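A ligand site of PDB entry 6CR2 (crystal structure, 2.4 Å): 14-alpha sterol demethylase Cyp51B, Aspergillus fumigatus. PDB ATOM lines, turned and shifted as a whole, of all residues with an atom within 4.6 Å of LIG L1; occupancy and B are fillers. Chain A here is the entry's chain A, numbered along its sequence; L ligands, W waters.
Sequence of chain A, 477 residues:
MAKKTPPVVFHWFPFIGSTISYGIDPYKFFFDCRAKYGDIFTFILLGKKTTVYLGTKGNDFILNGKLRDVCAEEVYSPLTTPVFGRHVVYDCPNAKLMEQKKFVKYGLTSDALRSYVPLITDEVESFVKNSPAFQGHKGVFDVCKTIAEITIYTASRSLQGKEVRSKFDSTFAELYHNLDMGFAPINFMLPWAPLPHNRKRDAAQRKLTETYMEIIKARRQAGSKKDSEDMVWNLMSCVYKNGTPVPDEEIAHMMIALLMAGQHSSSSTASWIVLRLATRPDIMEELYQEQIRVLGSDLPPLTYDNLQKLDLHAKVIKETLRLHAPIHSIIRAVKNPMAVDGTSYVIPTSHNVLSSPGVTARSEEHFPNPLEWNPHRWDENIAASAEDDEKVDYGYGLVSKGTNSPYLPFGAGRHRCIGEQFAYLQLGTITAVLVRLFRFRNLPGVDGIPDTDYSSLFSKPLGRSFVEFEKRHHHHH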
ATOM      1  N   LEU A  63     -11.547  24.591  26.285  1.00  0.00           N
ATOM      2  CA  LEU A  63     -12.497  23.557  26.718  1.00  0.00           C
ATOM      3  C   LEU A  63     -11.996  22.795  27.940  1.00  0.00           C
ATOM      4  O   LEU A  63     -12.796  22.245  28.705  1.00  0.00           O
ATOM      5  CB  LEU A  63     -12.778  22.582  25.566  1.00  0.00           C
ATOM      6  CG  LEU A  63     -13.370  23.226  24.307  1.00  0.00           C
ATOM      7  CD1 LEU A  63     -13.349  22.264  23.140  1.00  0.00           C
ATOM      8  CD2 LEU A  63     -14.788  23.722  24.567  1.00  0.00           C
ATOM      9  N   TYR A  76     -24.017  32.434  28.969  1.00  0.00           N
ATOM     10  CA  TYR A  76     -25.234  31.809  28.457  1.00  0.00           C
ATOM     11  C   TYR A  76     -26.491  32.193  29.223  1.00  0.00           C
ATOM     12  O   TYR A  76     -27.570  32.324  28.636  1.00  0.00           O
ATOM     13  CB  TYR A  76     -25.096  30.284  28.469  1.00  0.00           C
ATOM     14  CG  TYR A  76     -23.922  29.769  27.680  1.00  0.00           C
ATOM     15  CD1 TYR A  76     -23.313  30.554  26.707  1.00  0.00           C
ATOM     16  CD2 TYR A  76     -23.421  28.482  27.897  1.00  0.00           C
ATOM     17  CE1 TYR A  76     -22.231  30.075  25.976  1.00  0.00           C
ATOM     18  CE2 TYR A  76     -22.347  28.002  27.178  1.00  0.00           C
ATOM     19  CZ  TYR A  76     -21.763  28.802  26.213  1.00  0.00           C
ATOM     20  OH  TYR A  76     -20.689  28.327  25.485  1.00  0.00           O
ATOM     21  N   TYR A  90     -27.576  26.359  33.324  1.00  0.00           N
ATOM     22  CA  TYR A  90     -26.718  27.521  33.486  1.00  0.00           C
ATOM     23  C   TYR A  90     -27.238  28.558  34.478  1.00  0.00           C
ATOM     24  O   TYR A  90     -26.699  29.660  34.546  1.00  0.00           O
ATOM     25  CB  TYR A  90     -26.517  28.183  32.132  1.00  0.00           C
ATOM     26  CG  TYR A  90     -25.970  27.218  31.103  1.00  0.00           C
ATOM     27  CD1 TYR A  90     -24.909  26.394  31.417  1.00  0.00           C
ATOM     28  CD2 TYR A  90     -26.527  27.122  29.835  1.00  0.00           C
ATOM     29  CE1 TYR A  90     -24.397  25.490  30.495  1.00  0.00           C
ATOM     30  CE2 TYR A  90     -26.032  26.232  28.911  1.00  0.00           C
ATOM     31  CZ  TYR A  90     -24.969  25.423  29.244  1.00  0.00           C
ATOM     32  OH  TYR A  90     -24.460  24.530  28.330  1.00  0.00           O
ATOM     33  N   LEU A  97     -24.725  21.876  37.912  1.00  0.00           N
ATOM     34  CA  LEU A  97     -24.783  21.415  36.535  1.00  0.00           C
ATOM     35  C   LEU A  97     -24.204  20.005  36.418  1.00  0.00           C
ATOM     36  O   LEU A  97     -24.810  19.127  35.796  1.00  0.00           O
ATOM     37  CB  LEU A  97     -24.008  22.368  35.630  1.00  0.00           C
ATOM     38  CG  LEU A  97     -23.897  21.991  34.153  1.00  0.00           C
ATOM     39  CD1 LEU A  97     -25.259  21.935  33.474  1.00  0.00           C
ATOM     40  CD2 LEU A  97     -23.003  22.982  33.423  1.00  0.00           C
ATOM     41  N   LYS A 101     -26.230  16.819  35.093  1.00  0.00           N
ATOM     42  CA  LYS A 101     -25.702  16.016  33.986  1.00  0.00           C
ATOM     43  C   LYS A 101     -25.574  14.545  34.360  1.00  0.00           C
ATOM     44  O   LYS A 101     -25.925  13.667  33.574  1.00  0.00           O
ATOM     45  CB  LYS A 101     -24.338  16.567  33.561  1.00  0.00           C
ATOM     46  CG  LYS A 101     -24.451  17.884  32.822  1.00  0.00           C
ATOM     47  CD  LYS A 101     -23.099  18.416  32.396  1.00  0.00           C
ATOM     48  CE  LYS A 101     -22.485  17.574  31.290  1.00  0.00           C
ATOM     49  NZ  LYS A 101     -21.438  18.344  30.565  1.00  0.00           N
ATOM     50  N   LEU A 159     -37.758   9.648  24.982  1.00  0.00           N
ATOM     51  CA  LEU A 159     -37.052  10.284  26.078  1.00  0.00           C
ATOM     52  C   LEU A 159     -38.004  11.001  27.037  1.00  0.00           C
ATOM     53  O   LEU A 159     -37.862  10.902  28.256  1.00  0.00           O
ATOM     54  CB  LEU A 159     -36.027  11.256  25.512  1.00  0.00           C
ATOM     55  CG  LEU A 159     -34.840  11.656  26.403  1.00  0.00           C
ATOM     56  CD1 LEU A 159     -33.651  12.028  25.527  1.00  0.00           C
ATOM     57  CD2 LEU A 159     -35.250  12.816  27.306  1.00  0.00           C
ATOM     58  N   LEU A 258     -33.921  19.466  27.736  1.00  0.00           N
ATOM     59  CA  LEU A 258     -33.481  18.282  26.994  1.00  0.00           C
ATOM     60  C   LEU A 258     -34.221  18.193  25.672  1.00  0.00           C
ATOM     61  O   LEU A 258     -33.664  17.793  24.650  1.00  0.00           O
ATOM     62  CB  LEU A 258     -33.673  17.008  27.819  1.00  0.00           C
ATOM     63  CG  LEU A 258     -32.676  16.814  28.955  1.00  0.00           C
ATOM     64  CD1 LEU A 258     -33.049  15.607  29.809  1.00  0.00           C
ATOM     65  CD2 LEU A 258     -31.256  16.670  28.442  1.00  0.00           C
ATOM     66  N   ALA A 261     -32.490  20.853  23.503  1.00  0.00           N
ATOM     67  CA  ALA A 261     -31.186  20.346  23.107  1.00  0.00           C
ATOM     68  C   ALA A 261     -31.270  19.368  21.941  1.00  0.00           C
ATOM     69  O   ALA A 261     -30.608  19.537  20.917  1.00  0.00           O
ATOM     70  CB  ALA A 261     -30.510  19.682  24.294  1.00  0.00           C
ATOM     71  N   GLY A 262     -32.081  18.320  22.107  1.00  0.00           N
ATOM     72  CA  GLY A 262     -32.255  17.323  21.059  1.00  0.00           C
ATOM     73  C   GLY A 262     -32.797  17.939  19.783  1.00  0.00           C
ATOM     74  O   GLY A 262     -32.297  17.672  18.689  1.00  0.00           O
ATOM     75  N   SER A 265     -30.138  20.410  17.754  1.00  0.00           N
ATOM     76  CA  SER A 265     -28.956  19.696  17.278  1.00  0.00           C
ATOM     77  C   SER A 265     -29.301  18.549  16.325  1.00  0.00           C
ATOM     78  O   SER A 265     -28.766  18.451  15.231  1.00  0.00           O
ATOM     79  CB  SER A 265     -28.178  19.142  18.475  1.00  0.00           C
ATOM     80  OG  SER A 265     -28.945  18.176  19.184  1.00  0.00           O
ATOM     81  N   SER A 266     -30.206  17.675  16.763  1.00  0.00           N
ATOM     82  CA  SER A 266     -30.510  16.456  16.013  1.00  0.00           C
ATOM     83  C   SER A 266     -31.254  16.750  14.715  1.00  0.00           C
ATOM     84  O   SER A 266     -30.962  16.142  13.682  1.00  0.00           O
ATOM     85  CB  SER A 266     -31.343  15.496  16.867  1.00  0.00           C
ATOM     86  OG  SER A 266     -32.597  16.057  17.179  1.00  0.00           O
ATOM     87  N   THR A 269     -28.990  17.995  12.132  1.00  0.00           N
ATOM     88  CA  THR A 269     -28.065  16.959  11.680  1.00  0.00           C
ATOM     89  C   THR A 269     -28.741  15.948  10.765  1.00  0.00           C
ATOM     90  O   THR A 269     -28.216  15.594   9.712  1.00  0.00           O
ATOM     91  CB  THR A 269     -27.420  16.218  12.868  1.00  0.00           C
ATOM     92  OG1 THR A 269     -26.748  17.165  13.708  1.00  0.00           O
ATOM     93  CG2 THR A 269     -26.420  15.186  12.383  1.00  0.00           C
ATOM     94  N   LEU A 321     -21.600  14.949  10.822  1.00  0.00           N
ATOM     95  CA  LEU A 321     -21.182  15.775  11.953  1.00  0.00           C
ATOM     96  C   LEU A 321     -19.833  16.435  11.688  1.00  0.00           C
ATOM     97  O   LEU A 321     -19.582  17.532  12.176  1.00  0.00           O
ATOM     98  CB  LEU A 321     -21.161  14.982  13.261  1.00  0.00           C
ATOM     99  CG  LEU A 321     -22.581  14.735  13.792  1.00  0.00           C
ATOM    100  CD1 LEU A 321     -22.640  13.518  14.699  1.00  0.00           C
ATOM    101  CD2 LEU A 321     -23.112  15.971  14.496  1.00  0.00           C
ATOM    102  N   PRO A 326     -23.811  21.135  14.482  1.00  0.00           N
ATOM    103  CA  PRO A 326     -24.670  22.296  14.646  1.00  0.00           C
ATOM    104  C   PRO A 326     -24.048  23.426  15.459  1.00  0.00           C
ATOM    105  O   PRO A 326     -24.346  24.597  15.217  1.00  0.00           O
ATOM    106  CB  PRO A 326     -25.906  21.747  15.367  1.00  0.00           C
ATOM    107  CG  PRO A 326     -25.540  20.401  15.876  1.00  0.00           C
ATOM    108  CD  PRO A 326     -24.405  19.898  15.025  1.00  0.00           C
ATOM    109  N   ILE A 327     -23.201  23.077  16.418  1.00  0.00           N
ATOM    110  CA  ILE A 327     -22.515  24.093  17.219  1.00  0.00           C
ATOM    111  C   ILE A 327     -21.126  24.369  16.658  1.00  0.00           C
ATOM    112  O   ILE A 327     -20.251  23.510  16.669  1.00  0.00           O
ATOM    113  CB  ILE A 327     -22.428  23.693  18.699  1.00  0.00           C
ATOM    114  CG1 ILE A 327     -23.830  23.416  19.257  1.00  0.00           C
ATOM    115  CG2 ILE A 327     -21.789  24.808  19.513  1.00  0.00           C
ATOM    116  CD1 ILE A 327     -24.186  21.950  19.341  1.00  0.00           C
ATOM    117  N   ILE A 330     -18.054  27.755  20.619  1.00  0.00           N
ATOM    118  CA  ILE A 330     -18.165  27.560  22.061  1.00  0.00           C
ATOM    119  C   ILE A 330     -17.440  28.699  22.774  1.00  0.00           C
ATOM    120  O   ILE A 330     -16.239  28.923  22.582  1.00  0.00           O
ATOM    121  CB  ILE A 330     -17.597  26.208  22.508  1.00  0.00           C
ATOM    122  CG1 ILE A 330     -18.172  25.088  21.643  1.00  0.00           C
ATOM    123  CG2 ILE A 330     -17.923  25.956  23.974  1.00  0.00           C
ATOM    124  CD1 ILE A 330     -17.715  23.702  22.033  1.00  0.00           C
ATOM    125  N   ARG A 332     -16.633  31.136  26.223  1.00  0.00           N
ATOM    126  CA  ARG A 332     -16.513  31.237  27.671  1.00  0.00           C
ATOM    127  C   ARG A 332     -16.083  32.645  28.068  1.00  0.00           C
ATOM    128  O   ARG A 332     -15.416  33.344  27.300  1.00  0.00           O
ATOM    129  CB  ARG A 332     -15.508  30.216  28.216  1.00  0.00           C
ATOM    130  CG  ARG A 332     -15.700  28.798  27.695  1.00  0.00           C
ATOM    131  CD  ARG A 332     -16.805  28.040  28.404  1.00  0.00           C
ATOM    132  NE  ARG A 332     -16.714  26.612  28.088  1.00  0.00           N
ATOM    133  CZ  ARG A 332     -17.637  25.920  27.428  1.00  0.00           C
ATOM    134  NH1 ARG A 332     -18.753  26.498  27.010  1.00  0.00           N
ATOM    135  NH2 ARG A 332     -17.441  24.632  27.187  1.00  0.00           N
ATOM    136  N   PRO A 409     -17.259  17.066  17.688  1.00  0.00           N
ATOM    137  CA  PRO A 409     -18.580  17.641  17.444  1.00  0.00           C
ATOM    138  C   PRO A 409     -19.423  17.700  18.715  1.00  0.00           C
ATOM    139  O   PRO A 409     -20.372  18.487  18.778  1.00  0.00           O
ATOM    140  CB  PRO A 409     -19.202  16.673  16.438  1.00  0.00           C
ATOM    141  CG  PRO A 409     -18.479  15.389  16.668  1.00  0.00           C
ATOM    142  CD  PRO A 409     -17.065  15.827  16.913  1.00  0.00           C
ATOM    143  N   PHE A 410     -19.091  16.883  19.715  1.00  0.00           N
ATOM    144  CA  PHE A 410     -19.815  16.921  20.984  1.00  0.00           C
ATOM    145  C   PHE A 410     -19.028  17.640  22.072  1.00  0.00           C
ATOM    146  O   PHE A 410     -19.341  17.523  23.257  1.00  0.00           O
ATOM    147  CB  PHE A 410     -20.173  15.505  21.427  1.00  0.00           C
ATOM    148  CG  PHE A 410     -21.143  14.832  20.497  1.00  0.00           C
ATOM    149  CD1 PHE A 410     -22.502  15.007  20.654  1.00  0.00           C
ATOM    150  CD2 PHE A 410     -20.687  14.033  19.453  1.00  0.00           C
ATOM    151  CE1 PHE A 410     -23.406  14.409  19.793  1.00  0.00           C
ATOM    152  CE2 PHE A 410     -21.582  13.430  18.589  1.00  0.00           C
ATOM    153  CZ  PHE A 410     -22.944  13.611  18.762  1.00  0.00           C
ATOM    154  N   GLY A 411     -18.025  18.396  21.656  1.00  0.00           N
ATOM    155  CA  GLY A 411     -17.194  19.174  22.568  1.00  0.00           C
ATOM    156  C   GLY A 411     -16.186  18.371  23.352  1.00  0.00           C
ATOM    157  O   GLY A 411     -15.796  17.268  22.954  1.00  0.00           O
ATOM    158  N   ARG A 414     -15.391  19.721  30.830  1.00  0.00           N
ATOM    159  CA  ARG A 414     -16.461  19.516  31.810  1.00  0.00           C
ATOM    160  C   ARG A 414     -17.831  19.727  31.189  1.00  0.00           C
ATOM    161  O   ARG A 414     -18.809  19.116  31.613  1.00  0.00           O
ATOM    162  CB  ARG A 414     -16.282  20.415  33.032  1.00  0.00           C
ATOM    163  CG  ARG A 414     -16.362  21.915  32.781  1.00  0.00           C
ATOM    164  CD  ARG A 414     -16.069  22.717  34.039  1.00  0.00           C
ATOM    165  NE  ARG A 414     -14.897  22.254  34.774  1.00  0.00           N
ATOM    166  CZ  ARG A 414     -14.935  21.634  35.943  1.00  0.00           C
ATOM    167  NH1 ARG A 414     -16.091  21.370  36.533  1.00  0.00           N
ATOM    168  NH2 ARG A 414     -13.805  21.253  36.528  1.00  0.00           N
ATOM    169  N   HIS A 415     -17.908  20.584  30.167  1.00  0.00           N
ATOM    170  CA  HIS A 415     -19.187  20.959  29.577  1.00  0.00           C
ATOM    171  C   HIS A 415     -19.599  20.095  28.388  1.00  0.00           C
ATOM    172  O   HIS A 415     -20.584  20.400  27.720  1.00  0.00           O
ATOM    173  CB  HIS A 415     -19.176  22.419  29.137  1.00  0.00           C
ATOM    174  CG  HIS A 415     -19.238  23.399  30.258  1.00  0.00           C
ATOM    175  ND1 HIS A 415     -20.389  23.666  30.964  1.00  0.00           N
ATOM    176  CD2 HIS A 415     -18.277  24.200  30.785  1.00  0.00           C
ATOM    177  CE1 HIS A 415     -20.138  24.584  31.881  1.00  0.00           C
ATOM    178  NE2 HIS A 415     -18.868  24.927  31.798  1.00  0.00           N
ATOM    179  N   ARG A 416     -18.860  19.028  28.106  1.00  0.00           N
ATOM    180  CA  ARG A 416     -19.117  18.230  26.910  1.00  0.00           C
ATOM    181  C   ARG A 416     -20.452  17.498  26.954  1.00  0.00           C
ATOM    182  O   ARG A 416     -21.004  17.244  28.020  1.00  0.00           O
ATOM    183  CB  ARG A 416     -17.986  17.229  26.645  1.00  0.00           C
ATOM    184  CG  ARG A 416     -17.979  16.031  27.574  1.00  0.00           C
ATOM    185  CD  ARG A 416     -17.217  14.868  26.963  1.00  0.00           C
ATOM    186  NE  ARG A 416     -18.098  14.025  26.151  1.00  0.00           N
ATOM    187  CZ  ARG A 416     -17.881  13.704  24.885  1.00  0.00           C
ATOM    188  NH1 ARG A 416     -16.800  14.146  24.239  1.00  0.00           N
ATOM    189  NH2 ARG A 416     -18.751  12.940  24.251  1.00  0.00           N
ATOM    190  N   CYS A 417     -20.957  17.170  25.766  1.00  0.00           N
ATOM    191  CA  CYS A 417     -22.290  16.598  25.592  1.00  0.00           C
ATOM    192  C   CYS A 417     -22.440  15.271  26.313  1.00  0.00           C
ATOM    193  O   CYS A 417     -21.557  14.414  26.242  1.00  0.00           O
ATOM    194  CB  CYS A 417     -22.590  16.388  24.112  1.00  0.00           C
ATOM    195  SG  CYS A 417     -24.323  16.098  23.712  1.00  0.00           S
ATOM    196  N   ILE A 418     -23.558  15.097  27.006  1.00  0.00           N
ATOM    197  CA  ILE A 418     -23.947  13.799  27.546  1.00  0.00           C
ATOM    198  C   ILE A 418     -25.111  13.205  26.758  1.00  0.00           C
ATOM    199  O   ILE A 418     -25.664  12.167  27.130  1.00  0.00           O
ATOM    200  CB  ILE A 418     -24.326  13.881  29.041  1.00  0.00           C
ATOM    201  CG1 ILE A 418     -25.307  15.023  29.300  1.00  0.00           C
ATOM    202  CG2 ILE A 418     -23.070  14.073  29.886  1.00  0.00           C
ATOM    203  CD1 ILE A 418     -25.956  14.946  30.662  1.00  0.00           C
ATOM    204  N   GLY A 419     -25.481  13.875  25.680  1.00  0.00           N
ATOM    205  CA  GLY A 419     -26.545  13.384  24.803  1.00  0.00           C
ATOM    206  C   GLY A 419     -26.067  12.517  23.658  1.00  0.00           C
ATOM    207  O   GLY A 419     -26.868  12.045  22.851  1.00  0.00           O
ATOM    208  N   PHE A 422     -27.454   9.018  22.808  1.00  0.00           N
ATOM    209  CA  PHE A 422     -28.858   9.111  22.421  1.00  0.00           C
ATOM    210  C   PHE A 422     -28.973   9.706  21.026  1.00  0.00           C
ATOM    211  O   PHE A 422     -29.782   9.244  20.214  1.00  0.00           O
ATOM    212  CB  PHE A 422     -29.674   9.941  23.415  1.00  0.00           C
ATOM    213  CG  PHE A 422     -31.117  10.046  23.035  1.00  0.00           C
ATOM    214  CD1 PHE A 422     -31.986   8.994  23.281  1.00  0.00           C
ATOM    215  CD2 PHE A 422     -31.604  11.174  22.391  1.00  0.00           C
ATOM    216  CE1 PHE A 422     -33.314   9.065  22.903  1.00  0.00           C
ATOM    217  CE2 PHE A 422     -32.935  11.257  22.021  1.00  0.00           C
ATOM    218  CZ  PHE A 422     -33.791  10.203  22.277  1.00  0.00           C
ATOM    219  N   ALA A 423     -28.164  10.716  20.743  1.00  0.00           N
ATOM    220  CA  ALA A 423     -28.207  11.377  19.447  1.00  0.00           C
ATOM    221  C   ALA A 423     -27.890  10.369  18.344  1.00  0.00           C
ATOM    222  O   ALA A 423     -28.628  10.265  17.365  1.00  0.00           O
ATOM    223  CB  ALA A 423     -27.233  12.542  19.388  1.00  0.00           C
ATOM    224  N   LEU A 427     -30.582   9.376  15.375  1.00  0.00           N
ATOM    225  CA  LEU A 427     -30.072   9.620  14.034  1.00  0.00           C
ATOM    226  C   LEU A 427     -29.835   8.299  13.313  1.00  0.00           C
ATOM    227  O   LEU A 427     -30.203   8.136  12.145  1.00  0.00           O
ATOM    228  CB  LEU A 427     -28.770  10.412  14.073  1.00  0.00           C
ATOM    229  CG  LEU A 427     -28.877  11.831  14.630  1.00  0.00           C
ATOM    230  CD1 LEU A 427     -27.508  12.471  14.764  1.00  0.00           C
ATOM    231  CD2 LEU A 427     -29.783  12.686  13.748  1.00  0.00           C
HETATM  232  C1  LIG L   1     -23.216  19.751  25.468  1.00  0.00           C
HETATM  233  C2  LIG L   1     -23.168  18.947  20.686  1.00  0.00           C
HETATM  234  C3  LIG L   1     -27.141  16.181  21.148  1.00  0.00           C
HETATM  235  C4  LIG L   1     -27.467  17.454  25.819  1.00  0.00           C
HETATM  236  C5  LIG L   1     -22.850  19.737  24.132  1.00  0.00           C
HETATM  237  C6  LIG L   1     -21.714  20.409  23.616  1.00  0.00           C
HETATM  238  C7  LIG L   1     -21.700  20.178  22.276  1.00  0.00           C
HETATM  239  C8  LIG L   1     -22.822  19.390  21.956  1.00  0.00           C
HETATM  240  C9  LIG L   1     -20.664  20.695  21.313  1.00  0.00           C
HETATM  241  C10 LIG L   1     -20.706  21.211  24.379  1.00  0.00           C
HETATM  242  C11 LIG L   1     -21.191  22.664  24.487  1.00  0.00           C
HETATM  243  C12 LIG L   1     -20.215  23.552  25.221  1.00  0.00           C
HETATM  244  O1  LIG L   1     -20.603  24.669  25.639  1.00  0.00           O
HETATM  245  O2  LIG L   1     -19.028  23.198  25.413  1.00  0.00           O
HETATM  246  C13 LIG L   1     -24.254  18.101  20.460  1.00  0.00           C
HETATM  247  C14 LIG L   1     -24.484  17.536  19.172  1.00  0.00           C
HETATM  248  C15 LIG L   1     -25.600  16.750  19.276  1.00  0.00           C
HETATM  249  C16 LIG L   1     -26.014  16.862  20.696  1.00  0.00           C
HETATM  250  C17 LIG L   1     -23.664  17.761  17.924  1.00  0.00           C
HETATM  251  C18 LIG L   1     -26.290  15.908  18.289  1.00  0.00           C
HETATM  252  C19 LIG L   1     -25.813  15.685  17.059  1.00  0.00           C
HETATM  253  C20 LIG L   1     -27.590  16.274  22.462  1.00  0.00           C
HETATM  254  C21 LIG L   1     -28.735  15.643  22.991  1.00  0.00           C
HETATM  255  C22 LIG L   1     -28.824  16.024  24.318  1.00  0.00           C
HETATM  256  C23 LIG L   1     -27.730  16.881  24.586  1.00  0.00           C
HETATM  257  C24 LIG L   1     -29.651  14.732  22.220  1.00  0.00           C
HETATM  258  C25 LIG L   1     -29.813  15.619  25.338  1.00  0.00           C
HETATM  259  C26 LIG L   1     -30.741  14.688  25.118  1.00  0.00           C
HETATM  260  C27 LIG L   1     -26.286  18.169  26.047  1.00  0.00           C
HETATM  261  C28 LIG L   1     -25.940  18.595  27.413  1.00  0.00           C
HETATM  262  C29 LIG L   1     -24.760  19.257  27.314  1.00  0.00           C
HETATM  263  C30 LIG L   1     -24.407  19.164  25.894  1.00  0.00           C
HETATM  264  C31 LIG L   1     -26.738  18.398  28.678  1.00  0.00           C
HETATM  265  C32 LIG L   1     -23.978  19.849  28.453  1.00  0.00           C
HETATM  266  C33 LIG L   1     -23.925  21.383  28.529  1.00  0.00           C
HETATM  267  C34 LIG L   1     -22.949  21.825  29.575  1.00  0.00           C
HETATM  268  O3  LIG L   1     -22.649  23.032  29.683  1.00  0.00           O
HETATM  269  O4  LIG L   1     -22.412  20.996  30.356  1.00  0.00           O
HETATM  270  N1  LIG L   1     -23.559  19.164  23.098  1.00  0.00           N
HETATM  271  N2  LIG L   1     -25.169  17.686  21.332  1.00  0.00           N
HETATM  272  N3  LIG L   1     -27.012  17.056  23.436  1.00  0.00           N
HETATM  273  N4  LIG L   1     -25.333  18.526  25.173  1.00  0.00           N
HETATM  274 FE1  LIG L   1     -25.266  18.193  23.359  1.00  0.00          FE
HETATM  275  C1  LG2 L   2     -24.204  35.510  19.918  1.00  0.00           C
HETATM  276  C2  LG2 L   2     -24.125  35.965  21.232  1.00  0.00           C
HETATM  277  C3  LG2 L   2     -27.936  26.501  23.441  1.00  0.00           C
HETATM  278  C4  LG2 L   2     -27.594  22.376  27.077  1.00  0.00           C
HETATM  279  C5  LG2 L   2     -27.162  23.069  25.953  1.00  0.00           C
HETATM  280  C6  LG2 L   2     -24.970  33.899  22.086  1.00  0.00           C
HETATM  281  C7  LG2 L   2     -25.251  33.117  23.097  1.00  0.00           C
HETATM  282  C8  LG2 L   2     -24.025  35.566  17.627  1.00  0.00           C
HETATM  283  C9  LG2 L   2     -27.579  21.375  22.245  1.00  0.00           C
HETATM  284  C10 LG2 L   2     -27.311  20.116  22.162  1.00  0.00           C
HETATM  285  C11 LG2 L   2     -25.801  21.077  23.245  1.00  0.00           C
HETATM  286  N1  LG2 L   2     -24.860  33.334  24.310  1.00  0.00           N
HETATM  287  O1  LG2 L   2     -28.868  26.329  22.702  1.00  0.00           O
HETATM  288  C12 LG2 L   2     -29.453  23.084  25.214  1.00  0.00           C
HETATM  289  C13 LG2 L   2     -26.516  28.026  24.660  1.00  0.00           C
HETATM  290  C14 LG2 L   2     -26.021  29.307  24.791  1.00  0.00           C
HETATM  291  C15 LG2 L   2     -27.771  28.719  22.833  1.00  0.00           C
HETATM  292  C16 LG2 L   2     -27.224  29.971  22.923  1.00  0.00           C
HETATM  293  C17 LG2 L   2     -27.434  27.735  23.707  1.00  0.00           C
HETATM  294  C18 LG2 L   2     -28.128  23.428  25.013  1.00  0.00           C
HETATM  295  O2  LG2 L   2     -23.893  36.321  18.844  1.00  0.00           O
HETATM  296  N2  LG2 L   2     -26.179  19.903  22.793  1.00  0.00           N
HETATM  297  N3  LG2 L   2     -25.233  32.218  24.880  1.00  0.00           N
HETATM  298  C19 LG2 L   2     -25.864  31.548  23.951  1.00  0.00           C
HETATM  299  C20 LG2 L   2     -26.314  30.297  23.898  1.00  0.00           C
HETATM  300  C21 LG2 L   2     -28.910  22.001  27.318  1.00  0.00           C
HETATM  301  F1  LG2 L   2     -24.268  35.601  23.815  1.00  0.00           F
HETATM  302  C22 LG2 L   2     -29.840  22.376  26.352  1.00  0.00           C
HETATM  303  C23 LG2 L   2     -24.445  35.147  22.326  1.00  0.00           C
HETATM  304  F2  LG2 L   2     -25.463  36.593  16.453  1.00  0.00           F
HETATM  305  F3  LG2 L   2     -24.402  35.371  15.488  1.00  0.00           F
HETATM  306  F4  LG2 L   2     -23.678  37.042  16.093  1.00  0.00           F
HETATM  307  C24 LG2 L   2     -24.785  34.257  19.734  1.00  0.00           C
HETATM  308  C25 LG2 L   2     -25.133  33.456  20.792  1.00  0.00           C
HETATM  309 CL1  LG2 L   2     -30.616  23.533  24.012  1.00  0.00          CL
HETATM  310 CL2  LG2 L   2     -29.314  21.155  28.700  1.00  0.00          CL
HETATM  311  C26 LG2 L   2     -27.763  24.102  23.866  1.00  0.00           C
HETATM  312  C27 LG2 L   2     -26.548  23.401  23.257  1.00  0.00           C
HETATM  313  N4  LG2 L   2     -26.656  21.974  22.918  1.00  0.00           N
HETATM  314  N5  LG2 L   2     -27.316  25.487  24.072  1.00  0.00           N
HETATM  315  O3  LG2 L   2     -25.668  32.095  22.973  1.00  0.00           O
HETATM  316  C28 LG2 L   2     -24.403  36.238  16.350  1.00  0.00           C
HETATM  317  O   HOH W   1     -23.807  25.030  25.748  1.00  0.00           O
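A nitrogen (N2) of LG2 L2 is bound to an iron atom (FE1) of LIG L1 (2.0 Å).
The backbone carbonyl oxygen (O) of Phe 410 lies within hydrogen-bond range of the backbone NH (N) of Cys 417. SG of Cys 417 sits close to N of Gly 419, at 3.2 Å. NH1 of Arg 332 is in hydrogen-bond range of OH of Tyr 76. The backbone carbonyl oxygen (O) of Arg 416 lies within hydrogen-bond range of the side-chain amino group (NZ) of Lys 101. The side-chain amino group (NZ) of Lys 101 sits at hydrogen-bond distance from the backbone carbonyl oxygen (O) of Arg 414 (2.9 Å). O of Ser 265 sits at hydrogen-bond distance from OG1 of Thr 269 (2.8 Å). The backbone carbonyl oxygen of Gly 262 is in hydrogen-bond range of the side-chain hydroxyl of Ser 265. The side-chain hydroxyl of Ser 265 sits at hydrogen-bond distance from the backbone carbonyl oxygen of Ala 261 (2.8 Å).
Merely in contact with LIG L1: Phe 410 (3.2 Å), Ile 330 (3.3 Å), Ser 265 (3.3 Å), Pro 409 (3.4 Å), Ile 327 (3.4 Å), Gly 411 (3.5 Å), Gly 419 (3.5 Å), Leu 258 (3.6 Å), Tyr 76 (3.7 Å), Ala 423 (3.7 Å), Pro 326 (3.7 Å), Leu 97 (3.7 Å), Ile 418 (3.7 Å), Leu 321 (3.7 Å), Thr 269 (3.8 Å), Gly 262 (3.9 Å), Arg 416 (3.9 Å), Ala 261 (3.96 Å) and Leu 159 (3.96 Å). Hydrophobic or aromatic side chains within 4 Å of LIG L1: Tyr 90, Leu 97, Leu 159, Leu 258, Ala 261, Leu 321, Pro 326, Ile 327, Ile 330, Phe 410, His 415, Ile 418 and Ala 423. Within 4 Å of LIG L1: Tyr 76, Tyr 90, Leu 97, Lys 101, Leu 159, Leu 258, Ala 261, Gly 262, Ser 265, Thr 269, Leu 321, Pro 326, Ile 327, Ile 330, Arg 332, Pro 409, Phe 410, Gly 411, His 415, Arg 416, Cys 417, Ile 418, Gly 419 and Ala 423. Along chain A the residues within 4 Å of LIG L1 span positions 76 to 423.
Water W1 lies within hydrogen-bond range of OH of Tyr 90 (2.7 Å) and O1 of LIG L1 (3.2 Å).
An iron atom (FE1) of LIG L1 is bound by the side-chain sulfur (SG) of Cys 417 (2.3 Å). A ring nitrogen (ND1) of His 415 is in hydrogen-bond range of an oxygen (O3) of LIG L1 (2.7 Å). The side-chain hydroxyl (OH) of Tyr 90 is in hydrogen-bond range of an oxygen (O3) of LIG L1, 2.7 Å away. NH2 of Arg 332 is in salt-bridge range of O2 of LIG L1, 2.8 Å away. An oxygen (O4) of LIG L1 lies within salt-bridge range of the side-chain amino group (NZ) of Lys 101, 2.8 Å away.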
